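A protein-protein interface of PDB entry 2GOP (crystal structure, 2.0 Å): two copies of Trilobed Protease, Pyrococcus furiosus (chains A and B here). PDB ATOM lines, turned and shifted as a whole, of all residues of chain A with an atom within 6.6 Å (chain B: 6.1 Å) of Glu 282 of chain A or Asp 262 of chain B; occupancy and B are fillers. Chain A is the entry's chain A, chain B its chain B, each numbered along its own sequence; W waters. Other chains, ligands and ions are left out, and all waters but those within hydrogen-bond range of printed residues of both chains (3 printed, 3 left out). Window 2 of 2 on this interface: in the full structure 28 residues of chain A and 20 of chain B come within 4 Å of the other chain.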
ATOM      1  N   GLU A 242       3.368  21.901  19.428  1.00  0.00           N
ATOM      2  CA  GLU A 242       3.840  22.017  20.833  1.00  0.00           C
ATOM      3  C   GLU A 242       5.033  22.960  21.025  1.00  0.00           C
ATOM      4  O   GLU A 242       4.988  23.885  21.841  1.00  0.00           O
ATOM      5  CB  GLU A 242       4.197  20.655  21.455  1.00  0.00           C
ATOM      6  CG  GLU A 242       4.353  20.743  22.973  1.00  0.00           C
ATOM      7  CD  GLU A 242       4.818  19.469  23.646  1.00  0.00           C
ATOM      8  OE1 GLU A 242       5.042  18.454  22.946  1.00  0.00           O
ATOM      9  OE2 GLU A 242       4.969  19.491  24.894  1.00  0.00           O
ATOM     10  N   ASP A 262      11.610  16.192  18.037  1.00  0.00           N
ATOM     11  CA  ASP A 262      10.406  16.576  18.792  1.00  0.00           C
ATOM     12  C   ASP A 262      10.780  16.937  20.213  1.00  0.00           C
ATOM     13  O   ASP A 262      10.504  16.194  21.147  1.00  0.00           O
ATOM     14  CB  ASP A 262       9.363  15.448  18.763  1.00  0.00           C
ATOM     15  CG  ASP A 262       8.058  15.831  19.461  1.00  0.00           C
ATOM     16  OD1 ASP A 262       7.799  17.032  19.667  1.00  0.00           O
ATOM     17  OD2 ASP A 262       7.296  14.920  19.815  1.00  0.00           O
ATOM     18  N   ARG A 263      11.438  18.083  20.368  1.00  0.00           N
ATOM     19  CA  ARG A 263      11.881  18.555  21.670  1.00  0.00           C
ATOM     20  C   ARG A 263      11.727  20.056  21.686  1.00  0.00           C
ATOM     21  O   ARG A 263      11.806  20.690  20.643  1.00  0.00           O
ATOM     22  CB  ARG A 263      13.358  18.212  21.922  1.00  0.00           C
ATOM     23  CG  ARG A 263      13.707  16.748  21.918  1.00  0.00           C
ATOM     24  CD  ARG A 263      13.184  16.035  23.114  1.00  0.00           C
ATOM     25  NE  ARG A 263      13.674  14.655  23.135  1.00  0.00           N
ATOM     26  CZ  ARG A 263      13.232  13.704  23.946  1.00  0.00           C
ATOM     27  NH1 ARG A 263      12.286  13.950  24.837  1.00  0.00           N
ATOM     28  NH2 ARG A 263      13.757  12.501  23.869  1.00  0.00           N
ATOM     29  N   PHE A 280      15.273  20.930  25.575  1.00  0.00           N
ATOM     30  CA  PHE A 280      14.658  20.336  26.761  1.00  0.00           C
ATOM     31  C   PHE A 280      14.378  18.856  26.458  1.00  0.00           C
ATOM     32  O   PHE A 280      13.545  18.544  25.602  1.00  0.00           O
ATOM     33  CB  PHE A 280      13.349  21.041  27.112  1.00  0.00           C
ATOM     34  CG  PHE A 280      13.530  22.409  27.721  1.00  0.00           C
ATOM     35  CD1 PHE A 280      14.058  23.454  26.977  1.00  0.00           C
ATOM     36  CD2 PHE A 280      13.148  22.653  29.028  1.00  0.00           C
ATOM     37  CE1 PHE A 280      14.215  24.712  27.532  1.00  0.00           C
ATOM     38  CE2 PHE A 280      13.301  23.908  29.593  1.00  0.00           C
ATOM     39  CZ  PHE A 280      13.835  24.942  28.843  1.00  0.00           C
ATOM     40  N   GLU A 281      15.077  17.967  27.169  1.00  0.00           N
ATOM     41  CA  GLU A 281      15.057  16.530  26.913  1.00  0.00           C
ATOM     42  C   GLU A 281      14.987  15.761  28.223  1.00  0.00           C
ATOM     43  O   GLU A 281      15.968  15.740  28.970  1.00  0.00           O
ATOM     44  CB  GLU A 281      16.356  16.096  26.233  1.00  0.00           C
ATOM     45  CG  GLU A 281      16.596  16.643  24.868  1.00  0.00           C
ATOM     46  CD  GLU A 281      17.945  16.215  24.323  1.00  0.00           C
ATOM     47  OE1 GLU A 281      18.985  16.585  24.916  1.00  0.00           O
ATOM     48  OE2 GLU A 281      17.965  15.516  23.295  1.00  0.00           O
ATOM     49  N   GLU A 282      13.845  15.147  28.512  1.00  0.00           N
ATOM     50  CA  GLU A 282      13.747  14.158  29.594  1.00  0.00           C
ATOM     51  C   GLU A 282      14.242  14.659  30.957  1.00  0.00           C
ATOM     52  O   GLU A 282      14.968  13.956  31.671  1.00  0.00           O
ATOM     53  CB  GLU A 282      14.517  12.897  29.197  1.00  0.00           C
ATOM     54  CG  GLU A 282      13.980  12.212  27.944  1.00  0.00           C
ATOM     55  CD  GLU A 282      12.884  11.210  28.256  1.00  0.00           C
ATOM     56  OE1 GLU A 282      11.823  11.623  28.780  1.00  0.00           O
ATOM     57  OE2 GLU A 282      13.086  10.004  27.977  1.00  0.00           O
ATOM     58  N   GLY A 283      13.841  15.874  31.320  1.00  0.00           N
ATOM     59  CA  GLY A 283      14.190  16.434  32.615  1.00  0.00           C
ATOM     60  C   GLY A 283      15.478  17.225  32.610  1.00  0.00           C
ATOM     61  O   GLY A 283      15.792  17.893  33.588  1.00  0.00           O
ATOM     62  N   SER A 284      16.220  17.163  31.506  1.00  0.00           N
ATOM     63  CA  SER A 284      17.467  17.917  31.366  1.00  0.00           C
ATOM     64  C   SER A 284      17.324  19.012  30.316  1.00  0.00           C
ATOM     65  O   SER A 284      16.388  19.008  29.508  1.00  0.00           O
ATOM     66  CB  SER A 284      18.615  16.980  30.986  1.00  0.00           C
ATOM     67  OG  SER A 284      18.931  16.119  32.065  1.00  0.00           O
ATOM     68  N   ARG A 301      22.812  14.843  32.838  1.00  0.00           N
ATOM     69  CA  ARG A 301      21.710  15.058  33.780  1.00  0.00           C
ATOM     70  C   ARG A 301      21.925  16.391  34.494  1.00  0.00           C
ATOM     71  O   ARG A 301      22.417  16.456  35.615  1.00  0.00           O
ATOM     72  CB  ARG A 301      21.549  13.875  34.745  1.00  0.00           C
ATOM     73  CG  ARG A 301      21.036  12.619  34.029  1.00  0.00           C
ATOM     74  CD  ARG A 301      20.494  11.566  34.987  1.00  0.00           C
ATOM     75  NE  ARG A 301      19.969  10.388  34.283  1.00  0.00           N
ATOM     76  CZ  ARG A 301      18.795  10.331  33.649  1.00  0.00           C
ATOM     77  NH1 ARG A 301      17.985  11.385  33.611  1.00  0.00           N
ATOM     78  NH2 ARG A 301      18.420   9.203  33.048  1.00  0.00           N
ATOM     79  N   GLU B 242      10.224  19.141  30.300  1.00  0.00           N
ATOM     80  CA  GLU B 242       9.948  19.364  28.892  1.00  0.00           C
ATOM     81  C   GLU B 242       8.504  19.772  28.624  1.00  0.00           C
ATOM     82  O   GLU B 242       8.258  20.687  27.834  1.00  0.00           O
ATOM     83  CB  GLU B 242      10.283  18.096  28.108  1.00  0.00           C
ATOM     84  CG  GLU B 242      10.340  18.292  26.621  1.00  0.00           C
ATOM     85  CD  GLU B 242      10.575  17.008  25.861  1.00  0.00           C
ATOM     86  OE1 GLU B 242      11.041  16.012  26.461  1.00  0.00           O
ATOM     87  OE2 GLU B 242      10.302  17.015  24.644  1.00  0.00           O
ATOM     88  N   HIS B 243       7.555  19.112  29.285  1.00  0.00           N
ATOM     89  CA  HIS B 243       6.144  19.252  28.933  1.00  0.00           C
ATOM     90  C   HIS B 243       5.290  19.913  29.999  1.00  0.00           C
ATOM     91  O   HIS B 243       5.480  19.680  31.198  1.00  0.00           O
ATOM     92  CB  HIS B 243       5.532  17.880  28.668  1.00  0.00           C
ATOM     93  CG  HIS B 243       6.198  17.119  27.573  1.00  0.00           C
ATOM     94  ND1 HIS B 243       6.110  17.492  26.249  1.00  0.00           N
ATOM     95  CD2 HIS B 243       6.974  16.012  27.604  1.00  0.00           C
ATOM     96  CE1 HIS B 243       6.800  16.643  25.510  1.00  0.00           C
ATOM     97  NE2 HIS B 243       7.332  15.735  26.307  1.00  0.00           N
ATOM     98  N   LYS B 245       1.929  19.627  31.873  1.00  0.00           N
ATOM     99  CA  LYS B 245       1.062  18.506  32.235  1.00  0.00           C
ATOM    100  C   LYS B 245       0.032  18.969  33.267  1.00  0.00           C
ATOM    101  O   LYS B 245      -0.074  20.177  33.526  1.00  0.00           O
ATOM    102  CB  LYS B 245       1.896  17.350  32.781  1.00  0.00           C
ATOM    103  CG  LYS B 245       2.905  16.802  31.790  1.00  0.00           C
ATOM    104  CD  LYS B 245       3.606  15.586  32.370  1.00  0.00           C
ATOM    105  CE  LYS B 245       4.566  14.978  31.380  1.00  0.00           C
ATOM    106  NZ  LYS B 245       5.097  13.649  31.832  1.00  0.00           N
ATOM    107  N   LEU B 258      -0.710  12.698  34.445  1.00  0.00           N
ATOM    108  CA  LEU B 258       0.016  12.371  33.207  1.00  0.00           C
ATOM    109  C   LEU B 258       1.510  12.123  33.446  1.00  0.00           C
ATOM    110  O   LEU B 258       2.301  12.181  32.510  1.00  0.00           O
ATOM    111  CB  LEU B 258      -0.141  13.508  32.183  1.00  0.00           C
ATOM    112  CG  LEU B 258      -1.516  13.701  31.539  1.00  0.00           C
ATOM    113  CD1 LEU B 258      -1.673  15.114  31.010  1.00  0.00           C
ATOM    114  CD2 LEU B 258      -1.732  12.677  30.425  1.00  0.00           C
ATOM    115  N   ASP B 259       1.889  11.831  34.687  1.00  0.00           N
ATOM    116  CA  ASP B 259       3.304  11.719  35.070  1.00  0.00           C
ATOM    117  C   ASP B 259       4.128  10.784  34.184  1.00  0.00           C
ATOM    118  O   ASP B 259       5.318  11.030  33.965  1.00  0.00           O
ATOM    119  CB  ASP B 259       3.434  11.264  36.532  1.00  0.00           C
ATOM    120  CG  ASP B 259       3.017  12.340  37.535  1.00  0.00           C
ATOM    121  OD1 ASP B 259       2.966  13.529  37.158  1.00  0.00           O
ATOM    122  OD2 ASP B 259       2.749  11.986  38.708  1.00  0.00           O
ATOM    123  N   GLU B 260       3.512   9.717  33.679  1.00  0.00           N
ATOM    124  CA  GLU B 260       4.241   8.730  32.879  1.00  0.00           C
ATOM    125  C   GLU B 260       3.948   8.802  31.374  1.00  0.00           C
ATOM    126  O   GLU B 260       4.456   7.979  30.605  1.00  0.00           O
ATOM    127  CB  GLU B 260       4.018   7.316  33.419  1.00  0.00           C
ATOM    128  CG  GLU B 260       2.587   6.833  33.422  1.00  0.00           C
ATOM    129  CD  GLU B 260       2.447   5.490  34.107  1.00  0.00           C
ATOM    130  OE1 GLU B 260       2.780   4.461  33.482  1.00  0.00           O
ATOM    131  OE2 GLU B 260       2.002   5.464  35.270  1.00  0.00           O
ATOM    132  N   VAL B 261       3.149   9.789  30.960  1.00  0.00           N
ATOM    133  CA  VAL B 261       2.935  10.087  29.545  1.00  0.00           C
ATOM    134  C   VAL B 261       3.865  11.233  29.187  1.00  0.00           C
ATOM    135  O   VAL B 261       3.773  12.317  29.777  1.00  0.00           O
ATOM    136  CB  VAL B 261       1.470  10.488  29.255  1.00  0.00           C
ATOM    137  CG1 VAL B 261       1.243  10.654  27.761  1.00  0.00           C
ATOM    138  CG2 VAL B 261       0.504   9.450  29.820  1.00  0.00           C
ATOM    139  N   ASP B 262       4.770  10.986  28.240  1.00  0.00           N
ATOM    140  CA  ASP B 262       5.751  11.984  27.817  1.00  0.00           C
ATOM    141  C   ASP B 262       5.188  12.895  26.717  1.00  0.00           C
ATOM    142  O   ASP B 262       5.726  12.957  25.609  1.00  0.00           O
ATOM    143  CB  ASP B 262       7.041  11.304  27.345  1.00  0.00           C
ATOM    144  CG  ASP B 262       8.232  12.246  27.347  1.00  0.00           C
ATOM    145  OD1 ASP B 262       8.343  13.070  28.280  1.00  0.00           O
ATOM    146  OD2 ASP B 262       9.059  12.160  26.418  1.00  0.00           O
ATOM    147  N   ARG B 263       4.100  13.591  27.045  1.00  0.00           N
ATOM    148  CA  ARG B 263       3.412  14.480  26.121  1.00  0.00           C
ATOM    149  C   ARG B 263       3.025  15.770  26.831  1.00  0.00           C
ATOM    150  O   ARG B 263       2.980  15.810  28.063  1.00  0.00           O
ATOM    151  CB  ARG B 263       2.145  13.832  25.569  1.00  0.00           C
ATOM    152  CG  ARG B 263       2.358  12.544  24.793  1.00  0.00           C
ATOM    153  CD  ARG B 263       3.089  12.783  23.469  1.00  0.00           C
ATOM    154  NE  ARG B 263       2.946  11.614  22.605  1.00  0.00           N
ATOM    155  CZ  ARG B 263       3.711  11.325  21.557  1.00  0.00           C
ATOM    156  NH1 ARG B 263       4.717  12.111  21.197  1.00  0.00           N
ATOM    157  NH2 ARG B 263       3.467  10.222  20.867  1.00  0.00           N
ATOM    158  N   GLY B 264       2.729  16.796  26.030  1.00  0.00           N
ATOM    159  CA  GLY B 264       2.363  18.118  26.512  1.00  0.00           C
ATOM    160  C   GLY B 264       0.890  18.389  26.266  1.00  0.00           C
ATOM    161  O   GLY B 264       0.329  17.953  25.254  1.00  0.00           O
HETATM  162  O   HOH W   1       4.023  16.199  23.349  1.00  0.00           O
HETATM  163  O   HOH W   2       5.885  14.763  22.434  1.00  0.00           O
HETATM  164  O   HOH W   3      10.514  16.142  30.829  1.00  0.00           O
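OE1 of Glu 242 of chain B lies within salt-bridge range of NH1 of Arg 263 of chain A, at 2.9 Å. The side-chain carboxylate of Glu 242 of chain A lies within hydrogen-bond range of a ring nitrogen (ND1) of His 243 of chain B, at 2.7 Å.
A ring nitrogen (ND1) of His 243 of chain B is in hydrogen-bond range of the backbone NH of Gly 264 of chain B, 3.5 Å away. NE2 of His 243 of chain B sits at hydrogen-bond distance from O of Asp 262 of chain B (3.3 Å).
Among the printed residues, merely in contact across the chains: Phe 280 of chain A with Glu 242 of chain B, Glu 242 of chain A with Gly 264 of chain B, Glu 282 of chain A with Glu 242 of chain B, Asp 262 of chain A with Glu 242 of chain B and Glu 282 of chain A with Asp 262 of chain B.
Glu 282 of chain A touches just these residues of chain B: Glu 242 (3.6 Å) and Asp 262 (3.7 Å). Of the printed residues of chain A, His 243 of chain B touches Glu 242 (2.7 Å). Of the printed residues of chain B, Glu 242 of chain A touches His 243 (2.7 Å) and Gly 264 (3.4 Å). The nearest printed residue of chain B that does not touch Glu 282 of chain A is His 243 of chain B (6.6 Å).
Of the 9 printed residues of chain A, 5 touch a printed residue of chain B. Of the 10 printed residues of chain B, 4 touch a printed residue of chain A. Among the printed residues, 7 pairs touch across the chains. Among the printed residues, Asp or Glu carboxylates within 4 Å of a Lys or Arg side-chain nitrogen of the other chain: Arg 263 of chain A with Glu 242 of chain B (2.9 Å).
Asp 262 of chain A touches Glu 242 of chain B, but with the chains exchanged Glu 242 of chain A does not touch Asp 262 of chain B (6.1 Å). Arg 263 of chain A touches Glu 242 of chain B, but with the chains exchanged Glu 242 of chain A does not touch Arg 263 of chain B (4.6 Å). 3 positions are printed for both chains. Of the 7 pairs that touch across the chains among the printed residues, none has its exchanged pair printed and touching as well.
Water W1 bridges the side-chain carboxylate of Glu 242 of chain A (2.5 Å) and the backbone NH of Gly 264 of chain B (3.0 Å). Water W2 bridges OD2 of Asp 262 of chain A (3.0 Å) and NH1 of Arg 263 of chain B (3.2 Å). Water W3 bridges the backbone NH of Glu 242 of chain B and the backbone NH of Gly 283 of chain A.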
